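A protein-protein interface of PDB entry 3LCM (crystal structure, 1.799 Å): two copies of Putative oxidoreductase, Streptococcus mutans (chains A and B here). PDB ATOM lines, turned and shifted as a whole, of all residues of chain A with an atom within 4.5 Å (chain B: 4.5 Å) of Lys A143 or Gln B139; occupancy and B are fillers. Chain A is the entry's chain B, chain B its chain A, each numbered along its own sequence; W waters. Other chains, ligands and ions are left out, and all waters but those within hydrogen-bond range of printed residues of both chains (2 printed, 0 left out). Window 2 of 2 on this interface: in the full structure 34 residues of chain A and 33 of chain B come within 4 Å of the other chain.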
ATOM      1  N   MET A 135     -11.759   8.412  15.557  1.00  0.00           N
ATOM      2  CA  MET A 135     -13.013   9.169  15.468  1.00  0.00           C
ATOM      3  C   MET A 135     -13.035  10.410  14.564  1.00  0.00           C
ATOM      4  O   MET A 135     -14.087  10.758  14.015  1.00  0.00           O
ATOM      5  CB  MET A 135     -13.530   9.514  16.869  1.00  0.00           C
ATOM      6  CG  MET A 135     -14.018   8.287  17.634  1.00  0.00           C
ATOM      7  SD  MET A 135     -15.108   7.226  16.643  1.00  0.00           S
ATOM      8  CE  MET A 135     -16.623   8.175  16.718  1.00  0.00           C
ATOM      9  N   VAL A 138     -13.916   9.145  10.955  1.00  0.00           N
ATOM     10  CA  VAL A 138     -15.164   8.452  10.639  1.00  0.00           C
ATOM     11  C   VAL A 138     -16.360   9.392  10.550  1.00  0.00           C
ATOM     12  O   VAL A 138     -16.385  10.447  11.180  1.00  0.00           O
ATOM     13  CB  VAL A 138     -15.480   7.315  11.635  1.00  0.00           C
ATOM     14  CG1 VAL A 138     -14.342   6.305  11.674  1.00  0.00           C
ATOM     15  CG2 VAL A 138     -15.750   7.877  13.026  1.00  0.00           C
ATOM     16  N   GLN A 139     -17.300   9.051   9.672  1.00  0.00           N
ATOM     17  CA  GLN A 139     -18.553   9.766   9.460  1.00  0.00           C
ATOM     18  C   GLN A 139     -19.662   9.417  10.504  1.00  0.00           C
ATOM     19  O   GLN A 139     -19.755   8.283  10.887  1.00  0.00           O
ATOM     20  CB  GLN A 139     -19.084   9.430   8.075  1.00  0.00           C
ATOM     21  CG  GLN A 139     -18.455  10.199   6.966  1.00  0.00           C
ATOM     22  CD  GLN A 139     -19.430  10.972   6.159  1.00  0.00           C
ATOM     23  OE1 GLN A 139     -19.577  12.108   6.303  1.00  0.00           O
ATOM     24  NE2 GLN A 139     -20.097  10.311   5.323  1.00  0.00           N
ATOM     25  N   ASP A 140     -20.455  10.413  10.933  1.00  0.00           N
ATOM     26  CA  ASP A 140     -21.608  10.268  11.826  1.00  0.00           C
ATOM     27  C   ASP A 140     -21.195   9.867  13.245  1.00  0.00           C
ATOM     28  O   ASP A 140     -20.585  10.662  13.958  1.00  0.00           O
ATOM     29  CB  ASP A 140     -22.667   9.317  11.239  1.00  0.00           C
ATOM     30  CG  ASP A 140     -24.006   9.392  11.971  1.00  0.00           C
ATOM     31  OD1 ASP A 140     -24.090  10.039  13.033  1.00  0.00           O
ATOM     32  OD2 ASP A 140     -24.985   8.799  11.487  1.00  0.00           O
ATOM     33  N   TYR A 141     -21.528   8.648  13.654  1.00  0.00           N
ATOM     34  CA  TYR A 141     -21.263   8.207  15.025  1.00  0.00           C
ATOM     35  C   TYR A 141     -21.852   9.173  16.060  1.00  0.00           C
ATOM     36  O   TYR A 141     -21.222   9.475  17.077  1.00  0.00           O
ATOM     37  CB  TYR A 141     -19.760   8.029  15.258  1.00  0.00           C
ATOM     38  CG  TYR A 141     -19.193   6.694  14.813  1.00  0.00           C
ATOM     39  CD1 TYR A 141     -18.737   5.768  15.749  1.00  0.00           C
ATOM     40  CD2 TYR A 141     -19.093   6.365  13.462  1.00  0.00           C
ATOM     41  CE1 TYR A 141     -18.207   4.549  15.358  1.00  0.00           C
ATOM     42  CE2 TYR A 141     -18.564   5.139  13.058  1.00  0.00           C
ATOM     43  CZ  TYR A 141     -18.119   4.239  14.013  1.00  0.00           C
ATOM     44  OH  TYR A 141     -17.583   3.023  13.629  1.00  0.00           O
ATOM     45  N   GLY A 142     -23.064   9.652  15.794  1.00  0.00           N
ATOM     46  CA  GLY A 142     -23.726  10.584  16.689  1.00  0.00           C
ATOM     47  C   GLY A 142     -23.638  12.029  16.230  1.00  0.00           C
ATOM     48  O   GLY A 142     -24.440  12.867  16.647  1.00  0.00           O
ATOM     49  N   LYS A 143     -22.666  12.326  15.373  1.00  0.00           N
ATOM     50  CA  LYS A 143     -22.496  13.686  14.867  1.00  0.00           C
ATOM     51  C   LYS A 143     -23.678  14.146  13.983  1.00  0.00           C
ATOM     52  O   LYS A 143     -23.979  15.342  13.911  1.00  0.00           O
ATOM     53  CB  LYS A 143     -21.160  13.826  14.129  1.00  0.00           C
ATOM     54  CG  LYS A 143     -19.940  13.635  15.025  1.00  0.00           C
ATOM     55  CD  LYS A 143     -18.629  13.951  14.292  1.00  0.00           C
ATOM     56  CE  LYS A 143     -18.280  12.895  13.237  1.00  0.00           C
ATOM     57  NZ  LYS A 143     -17.757  11.621  13.830  1.00  0.00           N
ATOM     58  N   VAL A 144     -24.343  13.204  13.312  1.00  0.00           N
ATOM     59  CA  VAL A 144     -25.535  13.546  12.539  1.00  0.00           C
ATOM     60  C   VAL A 144     -26.658  14.006  13.461  1.00  0.00           C
ATOM     61  O   VAL A 144     -27.194  15.097  13.282  1.00  0.00           O
ATOM     62  CB  VAL A 144     -26.019  12.399  11.612  1.00  0.00           C
ATOM     63  CG1 VAL A 144     -27.423  12.696  11.078  1.00  0.00           C
ATOM     64  CG2 VAL A 144     -25.049  12.203  10.447  1.00  0.00           C
ATOM     65  N   LEU A 145     -27.005  13.191  14.453  1.00  0.00           N
ATOM     66  CA  LEU A 145     -28.060  13.575  15.394  1.00  0.00           C
ATOM     67  C   LEU A 145     -27.790  14.957  16.008  1.00  0.00           C
ATOM     68  O   LEU A 145     -28.674  15.815  16.070  1.00  0.00           O
ATOM     69  CB  LEU A 145     -28.219  12.524  16.500  1.00  0.00           C
ATOM     70  CG  LEU A 145     -29.275  12.813  17.583  1.00  0.00           C
ATOM     71  CD1 LEU A 145     -30.668  13.043  16.958  1.00  0.00           C
ATOM     72  CD2 LEU A 145     -29.313  11.719  18.649  1.00  0.00           C
ATOM     73  N   LYS A 146     -26.558  15.166  16.452  1.00  0.00           N
ATOM     74  CA  LYS A 146     -26.194  16.412  17.118  1.00  0.00           C
ATOM     75  C   LYS A 146     -26.161  17.614  16.169  1.00  0.00           C
ATOM     76  O   LYS A 146     -26.820  18.636  16.412  1.00  0.00           O
ATOM     77  CB  LYS A 146     -24.850  16.252  17.832  1.00  0.00           C
ATOM     78  CG  LYS A 146     -24.229  17.559  18.307  1.00  0.00           C
ATOM     79  CD  LYS A 146     -23.054  17.302  19.245  1.00  0.00           C
ATOM     80  CE  LYS A 146     -22.117  18.505  19.319  1.00  0.00           C
ATOM     81  NZ  LYS A 146     -22.720  19.715  19.945  1.00  0.00           N
ATOM     82  N   LYS A 147     -25.402  17.479  15.083  1.00  0.00           N
ATOM     83  CA  LYS A 147     -25.096  18.609  14.217  1.00  0.00           C
ATOM     84  C   LYS A 147     -26.116  18.842  13.109  1.00  0.00           C
ATOM     85  O   LYS A 147     -26.294  19.982  12.658  1.00  0.00           O
ATOM     86  CB  LYS A 147     -23.694  18.453  13.617  1.00  0.00           C
ATOM     87  N   GLN A 148     -26.790  17.776  12.675  1.00  0.00           N
ATOM     88  CA  GLN A 148     -27.681  17.863  11.515  1.00  0.00           C
ATOM     89  C   GLN A 148     -29.141  17.466  11.757  1.00  0.00           C
ATOM     90  O   GLN A 148     -29.935  17.425  10.818  1.00  0.00           O
ATOM     91  CB  GLN A 148     -27.078  17.091  10.334  1.00  0.00           C
ATOM     92  CG  GLN A 148     -25.780  17.740   9.844  1.00  0.00           C
ATOM     93  CD  GLN A 148     -24.949  16.865   8.934  1.00  0.00           C
ATOM     94  OE1 GLN A 148     -23.737  17.050   8.834  1.00  0.00           O
ATOM     95  NE2 GLN A 148     -25.589  15.920   8.254  1.00  0.00           N
ATOM     96  N   LEU A 160     -22.355  15.706  23.469  1.00  0.00           N
ATOM     97  CA  LEU A 160     -22.169  14.367  22.934  1.00  0.00           C
ATOM     98  C   LEU A 160     -21.110  13.602  23.721  1.00  0.00           C
ATOM     99  O   LEU A 160     -19.954  14.005  23.798  1.00  0.00           O
ATOM    100  CB  LEU A 160     -21.824  14.412  21.439  1.00  0.00           C
ATOM    101  CG  LEU A 160     -21.493  13.089  20.743  1.00  0.00           C
ATOM    102  CD1 LEU A 160     -22.599  12.052  20.941  1.00  0.00           C
ATOM    103  CD2 LEU A 160     -21.229  13.320  19.265  1.00  0.00           C
ATOM    104  N   SER B  86     -30.132  13.401   6.736  1.00  0.00           N
ATOM    105  CA  SER B  86     -28.737  13.142   6.368  1.00  0.00           C
ATOM    106  C   SER B  86     -28.392  11.703   5.982  1.00  0.00           C
ATOM    107  O   SER B  86     -27.224  11.401   5.755  1.00  0.00           O
ATOM    108  CB  SER B  86     -27.795  13.585   7.489  1.00  0.00           C
ATOM    109  OG  SER B  86     -27.998  14.944   7.800  1.00  0.00           O
ATOM    110  N   PHE B 137     -18.791  18.532   2.845  1.00  0.00           N
ATOM    111  CA  PHE B 137     -18.782  19.093   4.193  1.00  0.00           C
ATOM    112  C   PHE B 137     -19.789  18.468   5.156  1.00  0.00           C
ATOM    113  O   PHE B 137     -19.610  18.535   6.369  1.00  0.00           O
ATOM    114  CB  PHE B 137     -19.026  20.600   4.127  1.00  0.00           C
ATOM    115  CG  PHE B 137     -18.034  21.331   3.285  1.00  0.00           C
ATOM    116  CD1 PHE B 137     -16.731  21.509   3.727  1.00  0.00           C
ATOM    117  CD2 PHE B 137     -18.398  21.846   2.053  1.00  0.00           C
ATOM    118  CE1 PHE B 137     -15.814  22.187   2.952  1.00  0.00           C
ATOM    119  CE2 PHE B 137     -17.483  22.526   1.279  1.00  0.00           C
ATOM    120  CZ  PHE B 137     -16.190  22.692   1.727  1.00  0.00           C
ATOM    121  N   VAL B 138     -20.864  17.894   4.630  1.00  0.00           N
ATOM    122  CA  VAL B 138     -21.881  17.296   5.491  1.00  0.00           C
ATOM    123  C   VAL B 138     -21.501  15.871   5.884  1.00  0.00           C
ATOM    124  O   VAL B 138     -20.777  15.184   5.162  1.00  0.00           O
ATOM    125  CB  VAL B 138     -23.264  17.276   4.822  1.00  0.00           C
ATOM    126  CG1 VAL B 138     -23.820  18.679   4.724  1.00  0.00           C
ATOM    127  CG2 VAL B 138     -23.177  16.630   3.452  1.00  0.00           C
ATOM    128  N   GLN B 139     -21.982  15.443   7.045  1.00  0.00           N
ATOM    129  CA  GLN B 139     -21.817  14.069   7.485  1.00  0.00           C
ATOM    130  C   GLN B 139     -22.825  13.189   6.761  1.00  0.00           C
ATOM    131  O   GLN B 139     -23.977  13.588   6.565  1.00  0.00           O
ATOM    132  CB  GLN B 139     -22.036  13.967   8.991  1.00  0.00           C
ATOM    133  CG  GLN B 139     -21.050  14.771   9.813  1.00  0.00           C
ATOM    134  CD  GLN B 139     -19.710  14.091   9.912  1.00  0.00           C
ATOM    135  OE1 GLN B 139     -19.636  12.872  10.005  1.00  0.00           O
ATOM    136  NE2 GLN B 139     -18.638  14.876   9.901  1.00  0.00           N
ATOM    137  N   ASP B 140     -22.379  12.001   6.367  1.00  0.00           N
ATOM    138  CA  ASP B 140     -23.228  11.007   5.712  1.00  0.00           C
ATOM    139  C   ASP B 140     -23.717  11.453   4.325  1.00  0.00           C
ATOM    140  O   ASP B 140     -22.917  11.595   3.399  1.00  0.00           O
ATOM    141  CB  ASP B 140     -24.391  10.597   6.625  1.00  0.00           C
ATOM    142  CG  ASP B 140     -25.029   9.284   6.210  1.00  0.00           C
ATOM    143  OD1 ASP B 140     -24.824   8.860   5.060  1.00  0.00           O
ATOM    144  OD2 ASP B 140     -25.734   8.674   7.037  1.00  0.00           O
ATOM    145  N   TYR B 141     -25.024  11.683   4.187  1.00  0.00           N
ATOM    146  CA  TYR B 141     -25.645  11.888   2.872  1.00  0.00           C
ATOM    147  C   TYR B 141     -25.253  10.788   1.873  1.00  0.00           C
ATOM    148  O   TYR B 141     -24.924  11.076   0.714  1.00  0.00           O
ATOM    149  CB  TYR B 141     -25.295  13.266   2.303  1.00  0.00           C
ATOM    150  CG  TYR B 141     -26.189  14.380   2.786  1.00  0.00           C
ATOM    151  CD1 TYR B 141     -27.124  14.961   1.933  1.00  0.00           C
ATOM    152  CD2 TYR B 141     -26.107  14.851   4.090  1.00  0.00           C
ATOM    153  CE1 TYR B 141     -27.953  15.980   2.363  1.00  0.00           C
ATOM    154  CE2 TYR B 141     -26.932  15.873   4.528  1.00  0.00           C
ATOM    155  CZ  TYR B 141     -27.853  16.430   3.658  1.00  0.00           C
ATOM    156  OH  TYR B 141     -28.671  17.443   4.077  1.00  0.00           O
HETATM  157  O   HOH W   1     -25.146   7.545   9.335  1.00  0.00           O
HETATM  158  O   HOH W   2     -30.213  16.218   8.386  1.00  0.00           O
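O of Ser B86 lies within hydrogen-bond range of N of Tyr B141. The side-chain amino group of Lys A143 sits at hydrogen-bond distance from the backbone carbonyl oxygen of Val A138 (3.2 Å). N of Gly A142 lies within hydrogen-bond range of OD1 of Asp A140, at 3.0 Å. The side-chain amino group of Lys A143 is in hydrogen-bond range of the backbone carbonyl oxygen of Asp A140. The backbone NH of Val A144 is in hydrogen-bond range of the side-chain carboxylate of Asp A140 (3.2 Å).
Gln A139 touches Val B138, but with the chains exchanged Val A138 does not touch Gln B139 (4.2 Å). Gln A139 touches its own counterpart, Gln B139. Gln A139 touches Asp B140, and with the chains exchanged Asp A140 touches Gln B139.
The side-chain hydroxyl (OG) of Ser B86 lies within hydrogen-bond range of the side-chain amide nitrogen (NE2) of Gln A148 (2.6 Å). The backbone carbonyl oxygen (O) of Val B138 sits close to the side-chain amide oxygen (OE1) of Gln A139, 3.5 Å away. OE1 of Gln B139 sits at hydrogen-bond distance from N of Asp A140. The side-chain amide oxygen of Gln A148 sits at hydrogen-bond distance from the backbone NH of Gln B139, 3.0 Å away. The side-chain amide oxygen (OE1) of Gln A139 is in hydrogen-bond range of the backbone NH (N) of Asp B140 (2.8 Å).
Of the 13 printed residues of chain A, 5 touch a printed residue of chain B. Printed residues of chain A that touch a printed residue of chain B: Gln A139, Asp A140, Lys A143, Val A144 and Gln A148. Hydrophobic or aromatic side chains of chain A that line the printed part of chain B: Val A144. Among the printed residues, no Asp or Glu carboxylate lies within 4 Å of a Lys or Arg side-chain nitrogen of the other chain.
Among the printed residues, merely in contact across the chains: Gln A139 with Gln B139 (3.2 Å), Lys A143 with Gln B139 (3.5 Å), Val A144 with Ser B86 (3.7 Å), Val A144 with Gln B139 (3.8 Å), Gln A148 with Val B138 (3.8 Å) and Gln A148 with Tyr B141 (3.96 Å).
Water W1 lies within hydrogen-bond range of OD2 of Asp A140 and OD2 of Asp B140. Water W2 lies within hydrogen-bond range of OG of Ser B86 (2.6 Å) and O of Gln A148 (2.7 Å).
Val A138 touches none of the printed residues of chain B. Of the printed residues of chain B, Gln A139 touches Val B138 (3.5 Å), Gln B139 (3.2 Å) and Asp B140 (2.8 Å). Gly A142 touches none of the printed residues of chain B. Printed residues of chain B within 4 Å of Lys A143: Gln B139. Of the printed residues of chain A, Ser B86 touches Val A144 and Gln A148. Printed residues of chain A within 4 Å of Val B138: Gln A139 (3.5 Å) and Gln A148 (3.8 Å). Gln B139 touches five residues of chain A. Printed residues of chain A within 4 Å of Tyr B141: Gln A148. The nearest printed residue of chain B that does not touch Lys A143 is Ser B86 (7.3 Å).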
